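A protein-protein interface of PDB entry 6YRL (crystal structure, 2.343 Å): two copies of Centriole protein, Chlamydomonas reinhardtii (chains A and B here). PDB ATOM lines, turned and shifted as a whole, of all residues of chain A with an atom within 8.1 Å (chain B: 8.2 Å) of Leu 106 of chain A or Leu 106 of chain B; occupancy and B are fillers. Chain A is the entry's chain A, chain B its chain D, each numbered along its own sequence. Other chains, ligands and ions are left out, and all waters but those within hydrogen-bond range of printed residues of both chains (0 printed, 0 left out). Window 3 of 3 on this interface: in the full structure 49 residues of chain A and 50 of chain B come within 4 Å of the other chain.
Cys 99 of chain A touches its own counterpart, Cys 99 of chain B. Leu 102 of chain B touches its own counterpart, Leu 102 of chain A. Leu 102 of chain A touches Leu 106 of chain B, but with the chains exchanged Leu 106 of chain A does not touch Leu 102 of chain B (4.02 Å). Leu 106 of chain B touches its own counterpart, Leu 106 of chain A. Positions printed for both chains: 99, 100, 101, 102, 103, 104, 105, 106, 107, 108, 109, 110, 111, 112 and 113.
Printed residues of chain B within 4 Å of Cys 99 of chain A: Cys 99 (2.0 Å) and Leu 102 (3.6 Å). Of the printed residues of chain B, Leu 102 of chain A touches Cys 99, Leu 102, Arg 103 and Leu 106. Asp 104 of chain A touches none of the printed residues of chain B. Of the printed residues of chain B, Thr 105 of chain A touches Leu 106. Leu 106 of chain A touches one residue of chain B. No residue of chain B comes within 4 Å of Ala 107 of chain A. Of the printed residues of chain A, Leu 102 of chain B touches Cys 99 and Leu 102. Leu 106 of chain B touches three residues of chain A. The nearest printed residue of chain B that does not touch Leu 106 of chain A is Thr 105 of chain B (4.02 Å). The nearest residue of chain A that does not touch Leu 106 of chain B is Ala 109 of chain A (5.2 Å).
Cys 99 of chain A touches Leu 102 of chain B. Leu 102 of chain A touches Cys 99 of chain B (CD1 to O, 3.5 Å). Leu 102 of chain A touches Leu 102 of chain B. CG of Arg 103 of chain B touches CD1 of Leu 102 of chain A (3.7 Å). Leu 106 of chain B touches Leu 102 of chain A (CD1 to CD2, 3.6 Å). CG2 of Thr 105 of chain A touches CD1 of Leu 106 of chain B (3.5 Å). Leu 106 of chain B touches Leu 106 of chain A (CD2 to CD1, 3.7 Å).
The side-chain sulfur (SG) of Cys 99 of chain A forms a disulfide with the side-chain sulfur (SG) of Cys 99 of chain B, at 2.0 Å.
Of the 15 printed residues of chain B, 4 touch a printed residue of chain A. Printed residues of chain B that touch a printed residue of chain A: Cys 99, Leu 102, Arg 103 and Leu 106. Hydrophobic or aromatic side chains of chain B that line the printed part of chain A: Leu 102 and Leu 106. Of the 15 printed residues of chain A, 4 touch a printed residue of chain B. Printed residues of chain A that touch a printed residue of chain B: Cys 99, Leu 102, Thr 105 and Leu 106. Hydrophobic or aromatic side chains of chain A within 4 Å of the printed part of chain B: Leu 102 and Leu 106. Among the printed residues, 8 pairs touch across the chains. Among the printed residues, no Asp or Glu carboxylate lies within 4 Å of a Lys or Arg side-chain nitrogen of the other chain.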
ATOM      1  N   CYS A  99       9.303 -24.459  22.822  1.00  0.00           N
ATOM      2  CA  CYS A  99       8.179 -23.712  22.259  1.00  0.00           C
ATOM      3  C   CYS A  99       7.187 -23.294  23.339  1.00  0.00           C
ATOM      4  O   CYS A  99       6.716 -22.151  23.347  1.00  0.00           O
ATOM      5  CB  CYS A  99       7.480 -24.542  21.184  1.00  0.00           C
ATOM      6  SG  CYS A  99       8.151 -24.238  19.531  1.00  0.00           S
ATOM      7  N   ALA A 100       6.845 -24.207  24.251  1.00  0.00           N
ATOM      8  CA  ALA A 100       5.903 -23.867  25.314  1.00  0.00           C
ATOM      9  C   ALA A 100       6.425 -22.720  26.163  1.00  0.00           C
ATOM     10  O   ALA A 100       5.666 -21.814  26.528  1.00  0.00           O
ATOM     11  CB  ALA A 100       5.627 -25.089  26.187  1.00  0.00           C
ATOM     12  N   ASP A 101       7.721 -22.739  26.485  1.00  0.00           N
ATOM     13  CA  ASP A 101       8.295 -21.649  27.268  1.00  0.00           C
ATOM     14  C   ASP A 101       8.190 -20.324  26.520  1.00  0.00           C
ATOM     15  O   ASP A 101       7.753 -19.310  27.087  1.00  0.00           O
ATOM     16  CB  ASP A 101       9.752 -21.961  27.613  1.00  0.00           C
ATOM     17  CG  ASP A 101       9.880 -23.042  28.670  1.00  0.00           C
ATOM     18  OD1 ASP A 101       8.846 -23.417  29.271  1.00  0.00           O
ATOM     19  OD2 ASP A 101      11.015 -23.514  28.902  1.00  0.00           O
ATOM     20  N   LEU A 102       8.579 -20.317  25.241  1.00  0.00           N
ATOM     21  CA  LEU A 102       8.457 -19.101  24.439  1.00  0.00           C
ATOM     22  C   LEU A 102       7.029 -18.569  24.450  1.00  0.00           C
ATOM     23  O   LEU A 102       6.795 -17.374  24.662  1.00  0.00           O
ATOM     24  CB  LEU A 102       8.899 -19.382  23.012  1.00  0.00           C
ATOM     25  CG  LEU A 102      10.406 -19.365  22.874  1.00  0.00           C
ATOM     26  CD1 LEU A 102      10.802 -19.989  21.546  1.00  0.00           C
ATOM     27  CD2 LEU A 102      10.880 -17.933  22.987  1.00  0.00           C
ATOM     28  N   ARG A 103       6.062 -19.456  24.228  1.00  0.00           N
ATOM     29  CA  ARG A 103       4.661 -19.057  24.193  1.00  0.00           C
ATOM     30  C   ARG A 103       4.201 -18.498  25.537  1.00  0.00           C
ATOM     31  O   ARG A 103       3.419 -17.537  25.576  1.00  0.00           O
ATOM     32  CB  ARG A 103       3.830 -20.262  23.745  1.00  0.00           C
ATOM     33  CG  ARG A 103       2.392 -20.287  24.178  1.00  0.00           C
ATOM     34  CD  ARG A 103       1.596 -21.210  23.262  1.00  0.00           C
ATOM     35  NE  ARG A 103       1.981 -21.039  21.861  1.00  0.00           N
ATOM     36  CZ  ARG A 103       1.304 -20.296  20.991  1.00  0.00           C
ATOM     37  NH1 ARG A 103       1.718 -20.193  19.735  1.00  0.00           N
ATOM     38  NH2 ARG A 103       0.211 -19.653  21.378  1.00  0.00           N
ATOM     39  N   ASP A 104       4.692 -19.061  26.644  1.00  0.00           N
ATOM     40  CA  ASP A 104       4.422 -18.465  27.949  1.00  0.00           C
ATOM     41  C   ASP A 104       4.943 -17.034  28.010  1.00  0.00           C
ATOM     42  O   ASP A 104       4.226 -16.121  28.437  1.00  0.00           O
ATOM     43  CB  ASP A 104       5.043 -19.317  29.060  1.00  0.00           C
ATOM     44  CG  ASP A 104       4.185 -20.515  29.433  1.00  0.00           C
ATOM     45  OD1 ASP A 104       2.973 -20.502  29.140  1.00  0.00           O
ATOM     46  OD2 ASP A 104       4.730 -21.478  30.015  1.00  0.00           O
ATOM     47  N   THR A 105       6.187 -16.816  27.562  1.00  0.00           N
ATOM     48  CA  THR A 105       6.784 -15.481  27.648  1.00  0.00           C
ATOM     49  C   THR A 105       6.008 -14.470  26.811  1.00  0.00           C
ATOM     50  O   THR A 105       5.686 -13.367  27.277  1.00  0.00           O
ATOM     51  CB  THR A 105       8.243 -15.532  27.200  1.00  0.00           C
ATOM     52  OG1 THR A 105       9.039 -16.135  28.229  1.00  0.00           O
ATOM     53  CG2 THR A 105       8.755 -14.136  26.937  1.00  0.00           C
ATOM     54  N   LEU A 106       5.710 -14.837  25.562  1.00  0.00           N
ATOM     55  CA  LEU A 106       4.900 -13.998  24.682  1.00  0.00           C
ATOM     56  C   LEU A 106       3.567 -13.641  25.332  1.00  0.00           C
ATOM     57  O   LEU A 106       3.202 -12.461  25.423  1.00  0.00           O
ATOM     58  CB  LEU A 106       4.670 -14.729  23.360  1.00  0.00           C
ATOM     59  CG  LEU A 106       4.427 -13.937  22.083  1.00  0.00           C
ATOM     60  CD1 LEU A 106       5.493 -12.875  21.899  1.00  0.00           C
ATOM     61  CD2 LEU A 106       4.403 -14.893  20.903  1.00  0.00           C
ATOM     62  N   ALA A 107       2.834 -14.658  25.804  1.00  0.00           N
ATOM     63  CA  ALA A 107       1.520 -14.426  26.405  1.00  0.00           C
ATOM     64  C   ALA A 107       1.607 -13.497  27.616  1.00  0.00           C
ATOM     65  O   ALA A 107       0.749 -12.622  27.799  1.00  0.00           O
ATOM     66  CB  ALA A 107       0.888 -15.763  26.789  1.00  0.00           C
ATOM     67  N   SER A 108       2.638 -13.668  28.451  1.00  0.00           N
ATOM     68  CA  SER A 108       2.839 -12.769  29.587  1.00  0.00           C
ATOM     69  C   SER A 108       3.052 -11.332  29.125  1.00  0.00           C
ATOM     70  O   SER A 108       2.477 -10.390  29.691  1.00  0.00           O
ATOM     71  CB  SER A 108       4.024 -13.248  30.428  1.00  0.00           C
ATOM     72  OG  SER A 108       4.200 -12.428  31.570  1.00  0.00           O
ATOM     73  N   ALA A 109       3.881 -11.141  28.091  1.00  0.00           N
ATOM     74  CA  ALA A 109       4.111  -9.794  27.575  1.00  0.00           C
ATOM     75  C   ALA A 109       2.819  -9.173  27.045  1.00  0.00           C
ATOM     76  O   ALA A 109       2.582  -7.969  27.222  1.00  0.00           O
ATOM     77  CB  ALA A 109       5.184  -9.823  26.489  1.00  0.00           C
ATOM     78  N   GLU A 110       1.970  -9.980  26.397  1.00  0.00           N
ATOM     79  CA  GLU A 110       0.641  -9.500  26.022  1.00  0.00           C
ATOM     80  C   GLU A 110      -0.135  -9.039  27.249  1.00  0.00           C
ATOM     81  O   GLU A 110      -0.765  -7.970  27.239  1.00  0.00           O
ATOM     82  CB  GLU A 110      -0.144 -10.592  25.292  1.00  0.00           C
ATOM     83  CG  GLU A 110      -1.662 -10.436  25.463  1.00  0.00           C
ATOM     84  CD  GLU A 110      -2.468 -11.612  24.928  1.00  0.00           C
ATOM     85  OE1 GLU A 110      -1.861 -12.621  24.508  1.00  0.00           O
ATOM     86  OE2 GLU A 110      -3.718 -11.527  24.944  1.00  0.00           O
ATOM     87  N   GLY A 111      -0.111  -9.841  28.320  1.00  0.00           N
ATOM     88  CA  GLY A 111      -0.828  -9.473  29.528  1.00  0.00           C
ATOM     89  C   GLY A 111      -0.405  -8.108  30.070  1.00  0.00           C
ATOM     90  O   GLY A 111      -1.250  -7.280  30.405  1.00  0.00           O
ATOM     91  N   ARG A 112       0.906  -7.876  30.138  1.00  0.00           N
ATOM     92  CA  ARG A 112       1.384  -6.593  30.667  1.00  0.00           C
ATOM     93  C   ARG A 112       1.053  -5.446  29.721  1.00  0.00           C
ATOM     94  O   ARG A 112       0.676  -4.353  30.167  1.00  0.00           O
ATOM     95  CB  ARG A 112       2.890  -6.647  30.937  1.00  0.00           C
ATOM     96  CG  ARG A 112       3.382  -7.951  31.521  1.00  0.00           C
ATOM     97  CD  ARG A 112       4.892  -7.933  31.816  1.00  0.00           C
ATOM     98  NE  ARG A 112       5.368  -6.703  32.451  1.00  0.00           N
ATOM     99  CZ  ARG A 112       6.160  -5.812  31.859  1.00  0.00           C
ATOM    100  NH1 ARG A 112       6.556  -6.003  30.610  1.00  0.00           N
ATOM    101  NH2 ARG A 112       6.550  -4.727  32.518  1.00  0.00           N
ATOM    102  N   ALA A 113       1.205  -5.665  28.411  1.00  0.00           N
ATOM    103  CA  ALA A 113       0.877  -4.613  27.452  1.00  0.00           C
ATOM    104  C   ALA A 113      -0.587  -4.200  27.570  1.00  0.00           C
ATOM    105  O   ALA A 113      -0.901  -3.005  27.642  1.00  0.00           O
ATOM    106  CB  ALA A 113       1.193  -5.072  26.028  1.00  0.00           C
ATOM    107  N   CYS B  99       9.198 -22.722  16.794  1.00  0.00           N
ATOM    108  CA  CYS B  99       9.940 -22.092  17.881  1.00  0.00           C
ATOM    109  C   CYS B  99      10.717 -20.875  17.391  1.00  0.00           C
ATOM    110  O   CYS B  99      10.686 -19.814  18.028  1.00  0.00           O
ATOM    111  CB  CYS B  99      10.882 -23.104  18.524  1.00  0.00           C
ATOM    112  SG  CYS B  99      10.166 -24.123  19.850  1.00  0.00           S
ATOM    113  N   ALA B 100      11.421 -21.005  16.261  1.00  0.00           N
ATOM    114  CA  ALA B 100      12.119 -19.855  15.688  1.00  0.00           C
ATOM    115  C   ALA B 100      11.166 -18.684  15.477  1.00  0.00           C
ATOM    116  O   ALA B 100      11.457 -17.546  15.878  1.00  0.00           O
ATOM    117  CB  ALA B 100      12.794 -20.246  14.371  1.00  0.00           C
ATOM    118  N   ASP B 101      10.006 -18.949  14.862  1.00  0.00           N
ATOM    119  CA  ASP B 101       9.031 -17.881  14.645  1.00  0.00           C
ATOM    120  C   ASP B 101       8.606 -17.251  15.967  1.00  0.00           C
ATOM    121  O   ASP B 101       8.437 -16.025  16.058  1.00  0.00           O
ATOM    122  CB  ASP B 101       7.816 -18.419  13.894  1.00  0.00           C
ATOM    123  CG  ASP B 101       8.138 -18.848  12.460  1.00  0.00           C
ATOM    124  OD1 ASP B 101       9.233 -18.527  11.938  1.00  0.00           O
ATOM    125  OD2 ASP B 101       7.280 -19.526  11.855  1.00  0.00           O
ATOM    126  N   LEU B 102       8.444 -18.072  17.013  1.00  0.00           N
ATOM    127  CA  LEU B 102       8.106 -17.522  18.325  1.00  0.00           C
ATOM    128  C   LEU B 102       9.196 -16.591  18.836  1.00  0.00           C
ATOM    129  O   LEU B 102       8.901 -15.517  19.373  1.00  0.00           O
ATOM    130  CB  LEU B 102       7.865 -18.644  19.325  1.00  0.00           C
ATOM    131  CG  LEU B 102       6.565 -19.402  19.124  1.00  0.00           C
ATOM    132  CD1 LEU B 102       6.545 -20.603  20.053  1.00  0.00           C
ATOM    133  CD2 LEU B 102       5.366 -18.484  19.364  1.00  0.00           C
ATOM    134  N   ARG B 103      10.462 -16.985  18.683  1.00  0.00           N
ATOM    135  CA  ARG B 103      11.555 -16.125  19.128  1.00  0.00           C
ATOM    136  C   ARG B 103      11.548 -14.792  18.390  1.00  0.00           C
ATOM    137  O   ARG B 103      11.785 -13.736  18.995  1.00  0.00           O
ATOM    138  CB  ARG B 103      12.894 -16.843  18.945  1.00  0.00           C
ATOM    139  CG  ARG B 103      13.318 -17.632  20.181  1.00  0.00           C
ATOM    140  CD  ARG B 103      14.687 -18.274  20.033  1.00  0.00           C
ATOM    141  NE  ARG B 103      14.742 -19.189  18.899  1.00  0.00           N
ATOM    142  CZ  ARG B 103      14.519 -20.498  18.983  1.00  0.00           C
ATOM    143  NH1 ARG B 103      14.213 -21.051  20.151  1.00  0.00           N
ATOM    144  NH2 ARG B 103      14.592 -21.255  17.895  1.00  0.00           N
ATOM    145  N   ASP B 104      11.244 -14.819  17.091  1.00  0.00           N
ATOM    146  CA  ASP B 104      11.193 -13.584  16.312  1.00  0.00           C
ATOM    147  C   ASP B 104      10.067 -12.667  16.789  1.00  0.00           C
ATOM    148  O   ASP B 104      10.286 -11.471  17.044  1.00  0.00           O
ATOM    149  CB  ASP B 104      11.016 -13.933  14.841  1.00  0.00           C
ATOM    150  CG  ASP B 104      12.285 -14.483  14.206  1.00  0.00           C
ATOM    151  OD1 ASP B 104      13.371 -14.342  14.809  1.00  0.00           O
ATOM    152  OD2 ASP B 104      12.179 -15.120  13.127  1.00  0.00           O
ATOM    153  N   THR B 105       8.846 -13.210  16.916  1.00  0.00           N
ATOM    154  CA  THR B 105       7.736 -12.404  17.431  1.00  0.00           C
ATOM    155  C   THR B 105       8.037 -11.872  18.829  1.00  0.00           C
ATOM    156  O   THR B 105       7.591 -10.772  19.190  1.00  0.00           O
ATOM    157  CB  THR B 105       6.437 -13.221  17.441  1.00  0.00           C
ATOM    158  OG1 THR B 105       6.284 -13.912  16.195  1.00  0.00           O
ATOM    159  CG2 THR B 105       5.227 -12.315  17.647  1.00  0.00           C
ATOM    160  N   LEU B 106       8.807 -12.630  19.616  1.00  0.00           N
ATOM    161  CA  LEU B 106       9.229 -12.161  20.933  1.00  0.00           C
ATOM    162  C   LEU B 106      10.126 -10.937  20.820  1.00  0.00           C
ATOM    163  O   LEU B 106       9.862  -9.898  21.443  1.00  0.00           O
ATOM    164  CB  LEU B 106       9.959 -13.275  21.678  1.00  0.00           C
ATOM    165  CG  LEU B 106       9.259 -13.740  22.949  1.00  0.00           C
ATOM    166  CD1 LEU B 106      10.243 -14.506  23.808  1.00  0.00           C
ATOM    167  CD2 LEU B 106       8.681 -12.553  23.696  1.00  0.00           C
ATOM    168  N   ALA B 107      11.207 -11.054  20.044  1.00  0.00           N
ATOM    169  CA  ALA B 107      12.118  -9.931  19.849  1.00  0.00           C
ATOM    170  C   ALA B 107      11.359  -8.676  19.441  1.00  0.00           C
ATOM    171  O   ALA B 107      11.489  -7.619  20.077  1.00  0.00           O
ATOM    172  CB  ALA B 107      13.168 -10.292  18.796  1.00  0.00           C
ATOM    173  N   SER B 108      10.527  -8.790  18.398  1.00  0.00           N
ATOM    174  CA  SER B 108       9.786  -7.625  17.917  1.00  0.00           C
ATOM    175  C   SER B 108       8.865  -7.064  18.996  1.00  0.00           C
ATOM    176  O   SER B 108       8.742  -5.841  19.142  1.00  0.00           O
ATOM    177  CB  SER B 108       8.991  -7.984  16.663  1.00  0.00           C
ATOM    178  OG  SER B 108       7.833  -8.737  16.985  1.00  0.00           O
ATOM    179  N   ALA B 109       8.222  -7.940  19.777  1.00  0.00           N
ATOM    180  CA  ALA B 109       7.296  -7.464  20.804  1.00  0.00           C
ATOM    181  C   ALA B 109       8.019  -6.663  21.882  1.00  0.00           C
ATOM    182  O   ALA B 109       7.572  -5.575  22.262  1.00  0.00           O
ATOM    183  CB  ALA B 109       6.540  -8.639  21.421  1.00  0.00           C
ATOM    184  N   GLU B 110       9.141  -7.187  22.395  1.00  0.00           N
ATOM    185  CA  GLU B 110       9.892  -6.459  23.419  1.00  0.00           C
ATOM    186  C   GLU B 110      10.421  -5.133  22.877  1.00  0.00           C
ATOM    187  O   GLU B 110      10.323  -4.086  23.546  1.00  0.00           O
ATOM    188  CB  GLU B 110      11.043  -7.322  23.937  1.00  0.00           C
ATOM    189  CG  GLU B 110      10.730  -8.103  25.209  1.00  0.00           C
ATOM    190  CD  GLU B 110      11.251  -9.532  25.164  1.00  0.00           C
ATOM    191  OE1 GLU B 110      12.117  -9.821  24.306  1.00  0.00           O
ATOM    192  OE2 GLU B 110      10.799 -10.360  25.988  1.00  0.00           O
ATOM    193  N   GLY B 111      10.989  -5.161  21.666  1.00  0.00           N
ATOM    194  CA  GLY B 111      11.385  -3.921  21.019  1.00  0.00           C
ATOM    195  C   GLY B 111      10.261  -2.901  20.983  1.00  0.00           C
ATOM    196  O   GLY B 111      10.477  -1.717  21.255  1.00  0.00           O
ATOM    197  N   ARG B 112       9.040  -3.351  20.667  1.00  0.00           N
ATOM    198  CA  ARG B 112       7.893  -2.448  20.708  1.00  0.00           C
ATOM    199  C   ARG B 112       7.593  -1.980  22.130  1.00  0.00           C
ATOM    200  O   ARG B 112       7.152  -0.841  22.323  1.00  0.00           O
ATOM    201  CB  ARG B 112       6.655  -3.120  20.100  1.00  0.00           C
ATOM    202  CG  ARG B 112       5.705  -2.153  19.370  1.00  0.00           C
ATOM    203  CD  ARG B 112       4.376  -2.799  18.954  1.00  0.00           C
ATOM    204  NE  ARG B 112       4.420  -4.258  18.994  1.00  0.00           N
ATOM    205  CZ  ARG B 112       3.578  -5.016  19.691  1.00  0.00           C
ATOM    206  NH1 ARG B 112       2.608  -4.454  20.406  1.00  0.00           N
ATOM    207  NH2 ARG B 112       3.700  -6.338  19.669  1.00  0.00           N
ATOM    208  N   ALA B 113       7.824  -2.832  23.137  1.00  0.00           N
ATOM    209  CA  ALA B 113       7.542  -2.441  24.517  1.00  0.00           C
ATOM    210  C   ALA B 113       8.434  -1.298  24.973  1.00  0.00           C
ATOM    211  O   ALA B 113       7.985  -0.434  25.740  1.00  0.00           O
ATOM    212  CB  ALA B 113       7.694  -3.636  25.457  1.00  0.00           C
